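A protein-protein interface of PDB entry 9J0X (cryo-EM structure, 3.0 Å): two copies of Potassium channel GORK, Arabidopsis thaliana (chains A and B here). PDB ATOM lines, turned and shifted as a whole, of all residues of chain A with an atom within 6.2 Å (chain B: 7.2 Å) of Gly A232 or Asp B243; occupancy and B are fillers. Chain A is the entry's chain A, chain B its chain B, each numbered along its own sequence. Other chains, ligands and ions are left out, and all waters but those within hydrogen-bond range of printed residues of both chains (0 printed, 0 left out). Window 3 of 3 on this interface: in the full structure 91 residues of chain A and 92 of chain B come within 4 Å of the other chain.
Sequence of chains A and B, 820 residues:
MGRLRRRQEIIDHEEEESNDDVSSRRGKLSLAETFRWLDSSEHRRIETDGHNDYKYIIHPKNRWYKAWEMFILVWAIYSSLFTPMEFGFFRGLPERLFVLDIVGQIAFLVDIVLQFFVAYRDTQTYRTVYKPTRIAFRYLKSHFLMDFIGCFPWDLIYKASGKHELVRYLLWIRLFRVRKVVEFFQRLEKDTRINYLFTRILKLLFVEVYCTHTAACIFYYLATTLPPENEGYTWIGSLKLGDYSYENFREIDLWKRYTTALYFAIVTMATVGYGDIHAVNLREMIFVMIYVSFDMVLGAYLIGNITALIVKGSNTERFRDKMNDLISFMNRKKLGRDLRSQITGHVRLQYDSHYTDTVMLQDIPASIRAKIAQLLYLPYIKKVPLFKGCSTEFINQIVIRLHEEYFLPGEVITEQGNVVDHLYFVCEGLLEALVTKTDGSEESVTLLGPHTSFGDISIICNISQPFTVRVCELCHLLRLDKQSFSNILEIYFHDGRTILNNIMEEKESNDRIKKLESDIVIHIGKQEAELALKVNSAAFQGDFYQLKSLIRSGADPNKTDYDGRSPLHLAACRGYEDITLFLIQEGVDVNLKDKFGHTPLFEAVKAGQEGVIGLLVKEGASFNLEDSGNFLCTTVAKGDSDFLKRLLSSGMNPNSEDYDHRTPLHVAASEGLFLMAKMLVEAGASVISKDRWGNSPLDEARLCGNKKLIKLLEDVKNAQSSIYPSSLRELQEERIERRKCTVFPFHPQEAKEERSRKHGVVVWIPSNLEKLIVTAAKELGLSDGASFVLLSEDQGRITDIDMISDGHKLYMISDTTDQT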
ATOM      1  N   PRO A 228     -25.984 -21.291 -11.413  1.00  0.00           N
ATOM      2  CA  PRO A 228     -27.090 -21.952 -12.126  1.00  0.00           C
ATOM      3  C   PRO A 228     -28.089 -20.995 -12.759  1.00  0.00           C
ATOM      4  O   PRO A 228     -28.888 -21.434 -13.593  1.00  0.00           O
ATOM      5  CB  PRO A 228     -27.755 -22.801 -11.035  1.00  0.00           C
ATOM      6  CG  PRO A 228     -27.304 -22.210  -9.752  1.00  0.00           C
ATOM      7  CD  PRO A 228     -25.928 -21.704 -10.002  1.00  0.00           C
ATOM      8  N   GLU A 229     -28.075 -19.712 -12.394  1.00  0.00           N
ATOM      9  CA  GLU A 229     -28.891 -18.739 -13.106  1.00  0.00           C
ATOM     10  C   GLU A 229     -28.329 -18.458 -14.492  1.00  0.00           C
ATOM     11  O   GLU A 229     -29.084 -18.128 -15.412  1.00  0.00           O
ATOM     12  CB  GLU A 229     -28.990 -17.442 -12.301  1.00  0.00           C
ATOM     13  CG  GLU A 229     -29.741 -17.569 -10.984  1.00  0.00           C
ATOM     14  CD  GLU A 229     -28.852 -18.003  -9.836  1.00  0.00           C
ATOM     15  OE1 GLU A 229     -27.625 -18.116 -10.042  1.00  0.00           O
ATOM     16  OE2 GLU A 229     -29.378 -18.239  -8.728  1.00  0.00           O
ATOM     17  N   ASN A 230     -27.015 -18.588 -14.659  1.00  0.00           N
ATOM     18  CA  ASN A 230     -26.336 -18.412 -15.941  1.00  0.00           C
ATOM     19  C   ASN A 230     -26.018 -19.747 -16.592  1.00  0.00           C
ATOM     20  O   ASN A 230     -24.955 -19.911 -17.192  1.00  0.00           O
ATOM     21  CB  ASN A 230     -25.063 -17.594 -15.761  1.00  0.00           C
ATOM     22  CG  ASN A 230     -25.337 -16.197 -15.255  1.00  0.00           C
ATOM     23  OD1 ASN A 230     -25.451 -15.255 -16.036  1.00  0.00           O
ATOM     24  ND2 ASN A 230     -25.435 -16.052 -13.940  1.00  0.00           N
ATOM     25  N   GLU A 231     -26.919 -20.724 -16.460  1.00  0.00           N
ATOM     26  CA  GLU A 231     -26.684 -22.048 -17.027  1.00  0.00           C
ATOM     27  C   GLU A 231     -26.708 -22.039 -18.545  1.00  0.00           C
ATOM     28  O   GLU A 231     -26.032 -22.858 -19.170  1.00  0.00           O
ATOM     29  CB  GLU A 231     -27.729 -23.038 -16.521  1.00  0.00           C
ATOM     30  CG  GLU A 231     -27.283 -23.885 -15.361  1.00  0.00           C
ATOM     31  CD  GLU A 231     -28.254 -25.006 -15.080  1.00  0.00           C
ATOM     32  OE1 GLU A 231     -29.244 -25.127 -15.831  1.00  0.00           O
ATOM     33  OE2 GLU A 231     -28.032 -25.758 -14.109  1.00  0.00           O
ATOM     34  N   GLY A 232     -27.474 -21.133 -19.154  1.00  0.00           N
ATOM     35  CA  GLY A 232     -27.592 -21.111 -20.600  1.00  0.00           C
ATOM     36  C   GLY A 232     -26.323 -20.711 -21.318  1.00  0.00           C
ATOM     37  O   GLY A 232     -26.153 -21.053 -22.490  1.00  0.00           O
ATOM     38  N   TYR A 233     -25.438 -19.988 -20.648  1.00  0.00           N
ATOM     39  CA  TYR A 233     -24.134 -19.638 -21.204  1.00  0.00           C
ATOM     40  C   TYR A 233     -23.061 -20.620 -20.747  1.00  0.00           C
ATOM     41  O   TYR A 233     -22.005 -20.223 -20.273  1.00  0.00           O
ATOM     42  CB  TYR A 233     -23.789 -18.205 -20.819  1.00  0.00           C
ATOM     43  CG  TYR A 233     -22.742 -17.545 -21.677  1.00  0.00           C
ATOM     44  CD1 TYR A 233     -22.743 -17.705 -23.054  1.00  0.00           C
ATOM     45  CD2 TYR A 233     -21.788 -16.711 -21.116  1.00  0.00           C
ATOM     46  CE1 TYR A 233     -21.795 -17.094 -23.840  1.00  0.00           C
ATOM     47  CE2 TYR A 233     -20.836 -16.091 -21.896  1.00  0.00           C
ATOM     48  CZ  TYR A 233     -20.846 -16.286 -23.258  1.00  0.00           C
ATOM     49  OH  TYR A 233     -19.903 -15.671 -24.043  1.00  0.00           O
ATOM     50  N   THR A 234     -23.319 -21.922 -20.888  1.00  0.00           N
ATOM     51  CA  THR A 234     -22.348 -22.970 -20.592  1.00  0.00           C
ATOM     52  C   THR A 234     -22.451 -24.040 -21.666  1.00  0.00           C
ATOM     53  O   THR A 234     -23.402 -24.072 -22.450  1.00  0.00           O
ATOM     54  CB  THR A 234     -22.562 -23.611 -19.215  1.00  0.00           C
ATOM     55  OG1 THR A 234     -23.954 -23.869 -19.013  1.00  0.00           O
ATOM     56  CG2 THR A 234     -22.044 -22.724 -18.103  1.00  0.00           C
ATOM     57  N   TRP A 235     -21.455 -24.925 -21.704  1.00  0.00           N
ATOM     58  CA  TRP A 235     -21.424 -25.930 -22.759  1.00  0.00           C
ATOM     59  C   TRP A 235     -22.446 -27.029 -22.532  1.00  0.00           C
ATOM     60  O   TRP A 235     -22.886 -27.667 -23.494  1.00  0.00           O
ATOM     61  CB  TRP A 235     -20.030 -26.540 -22.880  1.00  0.00           C
ATOM     62  CG  TRP A 235     -19.595 -27.420 -21.742  1.00  0.00           C
ATOM     63  CD1 TRP A 235     -18.899 -27.040 -20.639  1.00  0.00           C
ATOM     64  CD2 TRP A 235     -19.793 -28.835 -21.622  1.00  0.00           C
ATOM     65  NE1 TRP A 235     -18.659 -28.124 -19.836  1.00  0.00           N
ATOM     66  CE2 TRP A 235     -19.204 -29.238 -20.415  1.00  0.00           C
ATOM     67  CE3 TRP A 235     -20.420 -29.795 -22.415  1.00  0.00           C
ATOM     68  CZ2 TRP A 235     -19.221 -30.557 -19.984  1.00  0.00           C
ATOM     69  CZ3 TRP A 235     -20.436 -31.101 -21.986  1.00  0.00           C
ATOM     70  CH2 TRP A 235     -19.841 -31.473 -20.783  1.00  0.00           C
ATOM     71  N   GLY A 237     -25.151 -26.593 -20.138  1.00  0.00           N
ATOM     72  CA  GLY A 237     -26.443 -25.995 -19.862  1.00  0.00           C
ATOM     73  C   GLY A 237     -27.199 -25.622 -21.118  1.00  0.00           C
ATOM     74  O   GLY A 237     -28.432 -25.614 -21.125  1.00  0.00           O
ATOM     75  N   SER A 238     -26.478 -25.318 -22.195  1.00  0.00           N
ATOM     76  CA  SER A 238     -27.075 -25.023 -23.487  1.00  0.00           C
ATOM     77  C   SER A 238     -27.074 -26.229 -24.408  1.00  0.00           C
ATOM     78  O   SER A 238     -27.093 -26.067 -25.631  1.00  0.00           O
ATOM     79  CB  SER A 238     -26.341 -23.866 -24.155  1.00  0.00           C
ATOM     80  OG  SER A 238     -25.085 -24.290 -24.643  1.00  0.00           O
ATOM     81  N   VAL A 280     -19.188 -22.552 -25.577  1.00  0.00           N
ATOM     82  CA  VAL A 280     -19.902 -21.301 -25.783  1.00  0.00           C
ATOM     83  C   VAL A 280     -19.390 -20.176 -24.893  1.00  0.00           C
ATOM     84  O   VAL A 280     -19.636 -19.003 -25.209  1.00  0.00           O
ATOM     85  CB  VAL A 280     -21.423 -21.472 -25.593  1.00  0.00           C
ATOM     86  CG1 VAL A 280     -21.953 -22.580 -26.475  1.00  0.00           C
ATOM     87  CG2 VAL A 280     -21.766 -21.710 -24.160  1.00  0.00           C
ATOM     88  N   LYS B 240     -24.476 -17.188 -32.700  1.00  0.00           N
ATOM     89  CA  LYS B 240     -25.209 -17.294 -31.444  1.00  0.00           C
ATOM     90  C   LYS B 240     -24.708 -18.548 -30.747  1.00  0.00           C
ATOM     91  O   LYS B 240     -25.019 -19.660 -31.177  1.00  0.00           O
ATOM     92  CB  LYS B 240     -26.714 -17.357 -31.680  1.00  0.00           C
ATOM     93  CG  LYS B 240     -27.520 -17.593 -30.417  1.00  0.00           C
ATOM     94  CD  LYS B 240     -29.011 -17.575 -30.695  1.00  0.00           C
ATOM     95  CE  LYS B 240     -29.806 -17.883 -29.438  1.00  0.00           C
ATOM     96  NZ  LYS B 240     -29.679 -16.808 -28.418  1.00  0.00           N
ATOM     97  N   LEU B 241     -23.922 -18.370 -29.691  1.00  0.00           N
ATOM     98  CA  LEU B 241     -23.304 -19.480 -28.977  1.00  0.00           C
ATOM     99  C   LEU B 241     -23.901 -19.544 -27.580  1.00  0.00           C
ATOM    100  O   LEU B 241     -23.645 -18.669 -26.747  1.00  0.00           O
ATOM    101  CB  LEU B 241     -21.788 -19.312 -28.930  1.00  0.00           C
ATOM    102  CG  LEU B 241     -21.061 -19.719 -30.211  1.00  0.00           C
ATOM    103  CD1 LEU B 241     -19.571 -19.674 -30.017  1.00  0.00           C
ATOM    104  CD2 LEU B 241     -21.490 -21.098 -30.665  1.00  0.00           C
ATOM    105  N   GLY B 242     -24.687 -20.584 -27.322  1.00  0.00           N
ATOM    106  CA  GLY B 242     -25.380 -20.696 -26.058  1.00  0.00           C
ATOM    107  C   GLY B 242     -26.639 -19.860 -26.052  1.00  0.00           C
ATOM    108  O   GLY B 242     -27.519 -20.052 -26.895  1.00  0.00           O
ATOM    109  N   ASP B 243     -26.740 -18.929 -25.107  1.00  0.00           N
ATOM    110  CA  ASP B 243     -27.819 -17.956 -25.094  1.00  0.00           C
ATOM    111  C   ASP B 243     -27.343 -16.554 -25.434  1.00  0.00           C
ATOM    112  O   ASP B 243     -28.134 -15.608 -25.362  1.00  0.00           O
ATOM    113  CB  ASP B 243     -28.526 -17.956 -23.732  1.00  0.00           C
ATOM    114  CG  ASP B 243     -27.673 -17.376 -22.619  1.00  0.00           C
ATOM    115  OD1 ASP B 243     -26.433 -17.487 -22.678  1.00  0.00           O
ATOM    116  OD2 ASP B 243     -28.248 -16.806 -21.670  1.00  0.00           O
ATOM    117  N   TYR B 244     -26.075 -16.396 -25.796  1.00  0.00           N
ATOM    118  CA  TYR B 244     -25.495 -15.102 -26.120  1.00  0.00           C
ATOM    119  C   TYR B 244     -25.466 -14.938 -27.630  1.00  0.00           C
ATOM    120  O   TYR B 244     -24.877 -15.760 -28.337  1.00  0.00           O
ATOM    121  CB  TYR B 244     -24.087 -14.981 -25.542  1.00  0.00           C
ATOM    122  CG  TYR B 244     -23.452 -13.631 -25.748  1.00  0.00           C
ATOM    123  CD1 TYR B 244     -23.833 -12.544 -24.980  1.00  0.00           C
ATOM    124  CD2 TYR B 244     -22.466 -13.447 -26.705  1.00  0.00           C
ATOM    125  CE1 TYR B 244     -23.256 -11.307 -25.166  1.00  0.00           C
ATOM    126  CE2 TYR B 244     -21.881 -12.215 -26.897  1.00  0.00           C
ATOM    127  CZ  TYR B 244     -22.281 -11.151 -26.124  1.00  0.00           C
ATOM    128  OH  TYR B 244     -21.708  -9.919 -26.307  1.00  0.00           O
ATOM    129  N   SER B 245     -26.099 -13.880 -28.119  1.00  0.00           N
ATOM    130  CA  SER B 245     -26.122 -13.571 -29.539  1.00  0.00           C
ATOM    131  C   SER B 245     -25.101 -12.483 -29.823  1.00  0.00           C
ATOM    132  O   SER B 245     -25.086 -11.449 -29.150  1.00  0.00           O
ATOM    133  CB  SER B 245     -27.513 -13.119 -29.979  1.00  0.00           C
ATOM    134  OG  SER B 245     -27.531 -12.812 -31.360  1.00  0.00           O
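Gly A232 touches Gly B242. Tyr A233 touches Leu B241 (CE1 to O, 3.8 Å). CE1 of Tyr A233 touches CB of Tyr B244 (3.6 Å). CB of Ser A238 touches CA of Gly B242 (3.8 Å). C of Leu B241 touches CB of Val A280, at 3.7 Å. Val A280 touches Gly B242 (CG1 to N, 3.5 Å).
The backbone carbonyl oxygen (O) of Thr A234 lies within hydrogen-bond range of the side-chain hydroxyl (OG) of Ser A238 (2.8 Å).
No position is printed for both chains. Of the 8 pairs that touch across the chains among the printed residues, none has its exchanged pair printed and touching as well.
The backbone NH of Asp B243 sits at hydrogen-bond distance from the backbone carbonyl oxygen of Gly A232 (3.4 Å). The side-chain carboxylate (OD1) of Asp B243 lies close to the backbone NH (N) of Tyr A233, 3.4 Å away.
Glu A229 touches none of the printed residues of chain B. Glu A231 touches none of the printed residues of chain B. Of chain B, only Gly B242 (3.7 Å) and Asp B243 (3.4 Å) come within 4 Å of Gly A232. Printed residues of chain B within 4 Å of Tyr A233: Leu B241 (3.8 Å), Asp B243 (3.3 Å) and Tyr B244 (3.6 Å). Printed residues of chain B within 4 Å of Ser A238: Gly B242 (3.8 Å). Of the printed residues of chain B, Val A280 touches Leu B241 and Gly B242. Of the printed residues of chain A, Leu B241 touches Tyr A233 (3.8 Å) and Val A280 (3.7 Å). Of the printed residues of chain A, Gly B242 touches Gly A232 (3.7 Å), Ser A238 (3.8 Å) and Val A280 (3.5 Å). Asp B243 touches two residues of chain A. The nearest residue of chain A that does not touch Asp B243 is Ser A238 (5.0 Å). The nearest printed residue of chain B that does not touch Tyr A233 is Gly B242 (5.0 Å).
Of the 6 printed residues of chain B, 4 touch a printed residue of chain A. Along chain B the printed residues that touch a printed residue of chain A span positions 241 to 244. Printed residues of chain A that touch a printed residue of chain B: Gly A232, Tyr A233, Ser A238 and Val A280. Hydrophobic or aromatic side chains of chain A that line the printed part of chain B: Tyr A233 and Val A280. Among the printed residues, no Asp or Glu carboxylate lies within 4 Å of a Lys or Arg side-chain nitrogen of the other chain.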
